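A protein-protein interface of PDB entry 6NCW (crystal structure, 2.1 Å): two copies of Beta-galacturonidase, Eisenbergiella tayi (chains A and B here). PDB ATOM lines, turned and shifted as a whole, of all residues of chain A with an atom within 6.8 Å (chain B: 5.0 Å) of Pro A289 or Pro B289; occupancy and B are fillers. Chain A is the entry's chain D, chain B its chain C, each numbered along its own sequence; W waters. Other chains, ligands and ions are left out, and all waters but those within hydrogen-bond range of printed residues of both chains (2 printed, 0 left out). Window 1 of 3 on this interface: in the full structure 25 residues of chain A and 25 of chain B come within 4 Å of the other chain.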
ATOM      1  N   PRO A  40      12.524  17.310  16.318  1.00  0.00           N
ATOM      2  CA  PRO A  40      12.037  15.923  16.464  1.00  0.00           C
ATOM      3  C   PRO A  40      12.961  15.021  17.271  1.00  0.00           C
ATOM      4  O   PRO A  40      14.149  15.318  17.417  1.00  0.00           O
ATOM      5  CB  PRO A  40      11.932  15.427  15.008  1.00  0.00           C
ATOM      6  CG  PRO A  40      12.936  16.245  14.259  1.00  0.00           C
ATOM      7  CD  PRO A  40      12.947  17.613  14.936  1.00  0.00           C
ATOM      8  N   HIS A 281      16.843   3.832  13.666  1.00  0.00           N
ATOM      9  CA  HIS A 281      18.279   4.131  13.845  1.00  0.00           C
ATOM     10  C   HIS A 281      18.605   4.025  15.333  1.00  0.00           C
ATOM     11  O   HIS A 281      17.816   4.503  16.169  1.00  0.00           O
ATOM     12  CB  HIS A 281      18.630   5.527  13.325  1.00  0.00           C
ATOM     13  CG  HIS A 281      20.098   5.846  13.301  1.00  0.00           C
ATOM     14  ND1 HIS A 281      20.816   6.150  14.439  1.00  0.00           N
ATOM     15  CD2 HIS A 281      20.966   5.973  12.266  1.00  0.00           C
ATOM     16  CE1 HIS A 281      22.072   6.409  14.112  1.00  0.00           C
ATOM     17  NE2 HIS A 281      22.191   6.303  12.800  1.00  0.00           N
ATOM     18  N   PHE A 284      18.590   7.601  16.769  1.00  0.00           N
ATOM     19  CA  PHE A 284      17.518   8.538  16.464  1.00  0.00           C
ATOM     20  C   PHE A 284      16.144   7.900  16.490  1.00  0.00           C
ATOM     21  O   PHE A 284      15.147   8.606  16.270  1.00  0.00           O
ATOM     22  CB  PHE A 284      17.768   9.199  15.097  1.00  0.00           C
ATOM     23  CG  PHE A 284      19.140   9.781  14.967  1.00  0.00           C
ATOM     24  CD1 PHE A 284      19.608  10.690  15.914  1.00  0.00           C
ATOM     25  CD2 PHE A 284      19.995   9.370  13.944  1.00  0.00           C
ATOM     26  CE1 PHE A 284      20.901  11.209  15.833  1.00  0.00           C
ATOM     27  CE2 PHE A 284      21.277   9.890  13.839  1.00  0.00           C
ATOM     28  CZ  PHE A 284      21.735  10.811  14.793  1.00  0.00           C
ATOM     29  N   ALA A 287      13.169   8.989  14.365  1.00  0.00           N
ATOM     30  CA  ALA A 287      13.268  10.427  14.105  1.00  0.00           C
ATOM     31  C   ALA A 287      14.601  10.761  13.433  1.00  0.00           C
ATOM     32  O   ALA A 287      15.420  11.508  13.965  1.00  0.00           O
ATOM     33  CB  ALA A 287      13.095  11.206  15.406  1.00  0.00           C
ATOM     34  N   LEU A 288      14.821  10.180  12.257  1.00  0.00           N
ATOM     35  CA  LEU A 288      16.125  10.308  11.603  1.00  0.00           C
ATOM     36  C   LEU A 288      16.259  11.679  10.952  1.00  0.00           C
ATOM     37  O   LEU A 288      15.370  12.091  10.201  1.00  0.00           O
ATOM     38  CB  LEU A 288      16.319   9.229  10.549  1.00  0.00           C
ATOM     39  CG  LEU A 288      16.786   7.854  11.010  1.00  0.00           C
ATOM     40  CD1 LEU A 288      15.669   7.081  11.731  1.00  0.00           C
ATOM     41  CD2 LEU A 288      17.317   7.069   9.821  1.00  0.00           C
ATOM     42  N   PRO A 289      17.354  12.396  11.197  1.00  0.00           N
ATOM     43  CA  PRO A 289      17.568  13.682  10.529  1.00  0.00           C
ATOM     44  C   PRO A 289      17.965  13.499   9.074  1.00  0.00           C
ATOM     45  O   PRO A 289      18.375  12.423   8.637  1.00  0.00           O
ATOM     46  CB  PRO A 289      18.714  14.312  11.322  1.00  0.00           C
ATOM     47  CG  PRO A 289      19.490  13.109  11.835  1.00  0.00           C
ATOM     48  CD  PRO A 289      18.458  12.045  12.110  1.00  0.00           C
ATOM     49  N   PHE A 290      17.823  14.596   8.327  1.00  0.00           N
ATOM     50  CA  PHE A 290      18.234  14.667   6.929  1.00  0.00           C
ATOM     51  C   PHE A 290      19.566  13.970   6.649  1.00  0.00           C
ATOM     52  O   PHE A 290      19.680  13.193   5.699  1.00  0.00           O
ATOM     53  CB  PHE A 290      18.289  16.148   6.525  1.00  0.00           C
ATOM     54  CG  PHE A 290      19.070  16.426   5.275  1.00  0.00           C
ATOM     55  CD1 PHE A 290      18.450  16.379   4.029  1.00  0.00           C
ATOM     56  CD2 PHE A 290      20.415  16.800   5.349  1.00  0.00           C
ATOM     57  CE1 PHE A 290      19.162  16.661   2.855  1.00  0.00           C
ATOM     58  CE2 PHE A 290      21.134  17.091   4.190  1.00  0.00           C
ATOM     59  CZ  PHE A 290      20.495  17.019   2.936  1.00  0.00           C
ATOM     60  N   SER A 291      20.598  14.267   7.447  1.00  0.00           N
ATOM     61  CA  SER A 291      21.915  13.686   7.196  1.00  0.00           C
ATOM     62  C   SER A 291      21.882  12.168   7.309  1.00  0.00           C
ATOM     63  O   SER A 291      22.551  11.467   6.544  1.00  0.00           O
ATOM     64  CB  SER A 291      22.940  14.258   8.174  1.00  0.00           C
ATOM     65  OG  SER A 291      23.099  15.643   7.978  1.00  0.00           O
ATOM     66  N   ALA A 292      21.128  11.650   8.283  1.00  0.00           N
ATOM     67  CA  ALA A 292      21.002  10.212   8.465  1.00  0.00           C
ATOM     68  C   ALA A 292      20.189   9.586   7.336  1.00  0.00           C
ATOM     69  O   ALA A 292      20.489   8.463   6.890  1.00  0.00           O
ATOM     70  CB  ALA A 292      20.360   9.913   9.825  1.00  0.00           C
ATOM     71  N   MET A 293      19.169  10.308   6.847  1.00  0.00           N
ATOM     72  CA  MET A 293      18.405   9.832   5.692  1.00  0.00           C
ATOM     73  C   MET A 293      19.284   9.705   4.461  1.00  0.00           C
ATOM     74  O   MET A 293      19.296   8.662   3.798  1.00  0.00           O
ATOM     75  CB  MET A 293      17.250  10.782   5.372  1.00  0.00           C
ATOM     76  CG  MET A 293      16.102  10.691   6.309  1.00  0.00           C
ATOM     77  SD  MET A 293      14.933  12.008   5.919  1.00  0.00           S
ATOM     78  CE  MET A 293      13.773  11.772   7.262  1.00  0.00           C
ATOM     79  N   GLN A 294      20.006  10.779   4.113  1.00  0.00           N
ATOM     80  CA  GLN A 294      20.814  10.729   2.896  1.00  0.00           C
ATOM     81  C   GLN A 294      21.916   9.682   3.009  1.00  0.00           C
ATOM     82  O   GLN A 294      22.279   9.054   2.008  1.00  0.00           O
ATOM     83  CB  GLN A 294      21.400  12.107   2.575  1.00  0.00           C
ATOM     84  CG  GLN A 294      22.193  12.156   1.268  1.00  0.00           C
ATOM     85  CD  GLN A 294      21.388  11.719   0.053  1.00  0.00           C
ATOM     86  OE1 GLN A 294      20.160  11.653   0.090  1.00  0.00           O
ATOM     87  NE2 GLN A 294      22.083  11.418  -1.037  1.00  0.00           N
ATOM     88  N   HIS A 295      22.444   9.456   4.209  1.00  0.00           N
ATOM     89  CA  HIS A 295      23.471   8.421   4.365  1.00  0.00           C
ATOM     90  C   HIS A 295      22.928   7.047   3.982  1.00  0.00           C
ATOM     91  O   HIS A 295      23.566   6.299   3.232  1.00  0.00           O
ATOM     92  CB  HIS A 295      24.000   8.417   5.793  1.00  0.00           C
ATOM     93  CG  HIS A 295      25.227   7.585   5.976  1.00  0.00           C
ATOM     94  ND1 HIS A 295      25.186   6.299   6.462  1.00  0.00           N
ATOM     95  CD2 HIS A 295      26.532   7.856   5.738  1.00  0.00           C
ATOM     96  CE1 HIS A 295      26.411   5.807   6.513  1.00  0.00           C
ATOM     97  NE2 HIS A 295      27.245   6.728   6.068  1.00  0.00           N
ATOM     98  N   LEU A 318      10.151  14.446   4.063  1.00  0.00           N
ATOM     99  CA  LEU A 318      11.530  14.790   3.741  1.00  0.00           C
ATOM    100  C   LEU A 318      12.260  13.605   3.090  1.00  0.00           C
ATOM    101  O   LEU A 318      13.042  13.786   2.150  1.00  0.00           O
ATOM    102  CB  LEU A 318      12.232  15.253   5.020  1.00  0.00           C
ATOM    103  CG  LEU A 318      13.699  15.672   4.953  1.00  0.00           C
ATOM    104  CD1 LEU A 318      13.877  16.872   4.038  1.00  0.00           C
ATOM    105  CD2 LEU A 318      14.192  15.982   6.352  1.00  0.00           C
ATOM    106  N   LEU A 322      13.759  13.414  -0.845  1.00  0.00           N
ATOM    107  CA  LEU A 322      15.078  12.950  -1.263  1.00  0.00           C
ATOM    108  C   LEU A 322      14.970  11.871  -2.321  1.00  0.00           C
ATOM    109  O   LEU A 322      15.853  11.751  -3.179  1.00  0.00           O
ATOM    110  CB  LEU A 322      15.858  12.419  -0.055  1.00  0.00           C
ATOM    111  CG  LEU A 322      16.186  13.512   0.958  1.00  0.00           C
ATOM    112  CD1 LEU A 322      16.835  12.909   2.226  1.00  0.00           C
ATOM    113  CD2 LEU A 322      17.086  14.557   0.282  1.00  0.00           C
ATOM    114  N   PHE B 284      28.885  10.769  10.058  1.00  0.00           N
ATOM    115  CA  PHE B 284      28.740  12.165   9.703  1.00  0.00           C
ATOM    116  C   PHE B 284      30.072  12.896   9.622  1.00  0.00           C
ATOM    117  O   PHE B 284      30.085  14.078   9.272  1.00  0.00           O
ATOM    118  CB  PHE B 284      27.790  12.844  10.705  1.00  0.00           C
ATOM    119  CG  PHE B 284      26.461  12.130  10.844  1.00  0.00           C
ATOM    120  CD1 PHE B 284      25.696  11.848   9.727  1.00  0.00           C
ATOM    121  CD2 PHE B 284      26.007  11.700  12.083  1.00  0.00           C
ATOM    122  CE1 PHE B 284      24.478  11.175   9.838  1.00  0.00           C
ATOM    123  CE2 PHE B 284      24.784  11.034  12.212  1.00  0.00           C
ATOM    124  CZ  PHE B 284      24.028  10.761  11.083  1.00  0.00           C
ATOM    125  N   ALA B 287      30.581  16.657  10.148  1.00  0.00           N
ATOM    126  CA  ALA B 287      29.346  17.343   9.764  1.00  0.00           C
ATOM    127  C   ALA B 287      28.146  16.795  10.546  1.00  0.00           C
ATOM    128  O   ALA B 287      27.172  16.285   9.979  1.00  0.00           O
ATOM    129  CB  ALA B 287      29.129  17.216   8.254  1.00  0.00           C
ATOM    130  N   LEU B 288      28.202  16.908  11.872  1.00  0.00           N
ATOM    131  CA  LEU B 288      27.149  16.280  12.674  1.00  0.00           C
ATOM    132  C   LEU B 288      25.877  17.118  12.636  1.00  0.00           C
ATOM    133  O   LEU B 288      25.937  18.336  12.848  1.00  0.00           O
ATOM    134  CB  LEU B 288      27.590  16.077  14.122  1.00  0.00           C
ATOM    135  CG  LEU B 288      28.435  14.830  14.455  1.00  0.00           C
ATOM    136  CD1 LEU B 288      29.817  14.873  13.824  1.00  0.00           C
ATOM    137  CD2 LEU B 288      28.568  14.687  15.954  1.00  0.00           C
ATOM    138  N   PRO B 289      24.721  16.506  12.383  1.00  0.00           N
ATOM    139  CA  PRO B 289      23.458  17.245  12.422  1.00  0.00           C
ATOM    140  C   PRO B 289      23.029  17.571  13.843  1.00  0.00           C
ATOM    141  O   PRO B 289      23.514  17.006  14.827  1.00  0.00           O
ATOM    142  CB  PRO B 289      22.469  16.273  11.778  1.00  0.00           C
ATOM    143  CG  PRO B 289      23.026  14.933  12.120  1.00  0.00           C
ATOM    144  CD  PRO B 289      24.513  15.097  11.999  1.00  0.00           C
ATOM    145  N   PHE B 290      22.087  18.499  13.921  1.00  0.00           N
ATOM    146  CA  PHE B 290      21.431  18.862  15.172  1.00  0.00           C
ATOM    147  C   PHE B 290      21.085  17.656  16.042  1.00  0.00           C
ATOM    148  O   PHE B 290      21.414  17.631  17.228  1.00  0.00           O
ATOM    149  CB  PHE B 290      20.168  19.682  14.850  1.00  0.00           C
ATOM    150  CG  PHE B 290      19.189  19.774  15.992  1.00  0.00           C
ATOM    151  CD1 PHE B 290      19.395  20.673  17.029  1.00  0.00           C
ATOM    152  CD2 PHE B 290      18.053  18.975  16.017  1.00  0.00           C
ATOM    153  CE1 PHE B 290      18.488  20.777  18.086  1.00  0.00           C
ATOM    154  CE2 PHE B 290      17.144  19.063  17.071  1.00  0.00           C
ATOM    155  CZ  PHE B 290      17.371  19.968  18.113  1.00  0.00           C
ATOM    156  N   SER B 291      20.416  16.642  15.478  1.00  0.00           N
ATOM    157  CA  SER B 291      20.014  15.491  16.290  1.00  0.00           C
ATOM    158  C   SER B 291      21.219  14.776  16.893  1.00  0.00           C
ATOM    159  O   SER B 291      21.145  14.254  18.010  1.00  0.00           O
ATOM    160  CB  SER B 291      19.194  14.505  15.458  1.00  0.00           C
ATOM    161  OG  SER B 291      18.038  15.117  14.924  1.00  0.00           O
ATOM    162  N   ALA B 292      22.330  14.711  16.158  1.00  0.00           N
ATOM    163  CA  ALA B 292      23.512  14.020  16.671  1.00  0.00           C
ATOM    164  C   ALA B 292      24.219  14.843  17.748  1.00  0.00           C
ATOM    165  O   ALA B 292      24.722  14.285  18.731  1.00  0.00           O
ATOM    166  CB  ALA B 292      24.460  13.687  15.519  1.00  0.00           C
ATOM    167  N   MET B 293      24.262  16.167  17.577  1.00  0.00           N
ATOM    168  CA  MET B 293      24.795  17.053  18.608  1.00  0.00           C
ATOM    169  C   MET B 293      24.053  16.882  19.921  1.00  0.00           C
ATOM    170  O   MET B 293      24.664  16.676  20.972  1.00  0.00           O
ATOM    171  CB  MET B 293      24.681  18.503  18.149  1.00  0.00           C
ATOM    172  CG  MET B 293      25.528  18.822  16.959  1.00  0.00           C
ATOM    173  SD  MET B 293      25.299  20.548  16.489  1.00  0.00           S
ATOM    174  CE  MET B 293      26.630  20.693  15.282  1.00  0.00           C
HETATM  175  O   HOH W   1      15.211  14.134  13.234  1.00  0.00           O
HETATM  176  O   HOH W   2      16.711  14.281  17.472  1.00  0.00           O
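Phe A284 touches Phe B284 (CE2 to CZ, 3.99 Å).
Ser B291 touches Phe A284.
Phe A284 touches Ala B292 (CE1 to N, 3.8 Å).
Pro B289 touches Pro A289 (CG to CG, 3.99 Å).
Pro A289 touches Ser B291 (CB to OG, 3.8 Å).
CE1 of Phe B284 touches C of Ser A291 (3.8 Å).
OG of Ser A291 touches CB of Pro B289, 3.9 Å away.
Ala A292 touches Phe B284 (N to CE1, 3.7 Å).
Of the printed residues of chain B, Pro A289 touches Pro B289 (3.99 Å) and Ser B291 (3.8 Å).
Phe A290 touches none of the printed residues of chain B.
Met A293 touches none of the printed residues of chain B.
Of the printed residues of chain A, Phe B284 touches Phe A284 (3.99 Å), Ser A291 (3.8 Å) and Ala A292 (3.7 Å).
Printed residues of chain A within 4 Å of Pro B289: Pro A289 and Ser A291.
Printed residues of chain A within 4 Å of Ala B292: Phe A284 (3.8 Å).
The nearest printed residue of chain B that does not touch Pro A289 is Phe B284 (5.2 Å).
The nearest printed residue of chain A that does not touch Pro B289 is Phe A284 (5.1 Å).
The nearest printed residue of chain A that does not touch Ala B292 is Pro A289 (5.4 Å).
Phe B284 touches its own counterpart, Phe A284.
Phe A284 touches Ser B291, and with the chains exchanged Ser A291 touches Phe B284.
Pro B289 touches its own counterpart, Pro A289.
Pro A289 touches Ser B291, and with the chains exchanged Ser A291 touches Pro B289.
8 positions are printed for both chains.
Of the 8 pairs that touch across the chains among the printed residues, 8 have their exchanged pair printed and touching as well.
Of the 14 printed residues of chain A, 4 touch a printed residue of chain B.
Printed residues of chain A that touch a printed residue of chain B: Phe A284, Pro A289, Ser A291 and Ala A292.
Hydrophobic or aromatic side chains of chain A that line the printed part of chain B: Phe A284, Pro A289 and Ala A292.
Printed residues of chain B that touch a printed residue of chain A: Phe B284, Pro B289, Ser B291 and Ala B292.
Among the printed residues, 8 pairs touch across the chains.
Among the printed residues, no Asp or Glu carboxylate lies within 4 Å of a Lys or Arg side-chain nitrogen of the other chain.
Water W1 lies within hydrogen-bond range of O of Ala A287 (2.7 Å) and OG of Ser B291 (3.4 Å).
Water W2 bridges the backbone carbonyl oxygen (O) of Pro A40 (2.8 Å) and the side-chain hydroxyl (OG) of Ser B291 (3.0 Å).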
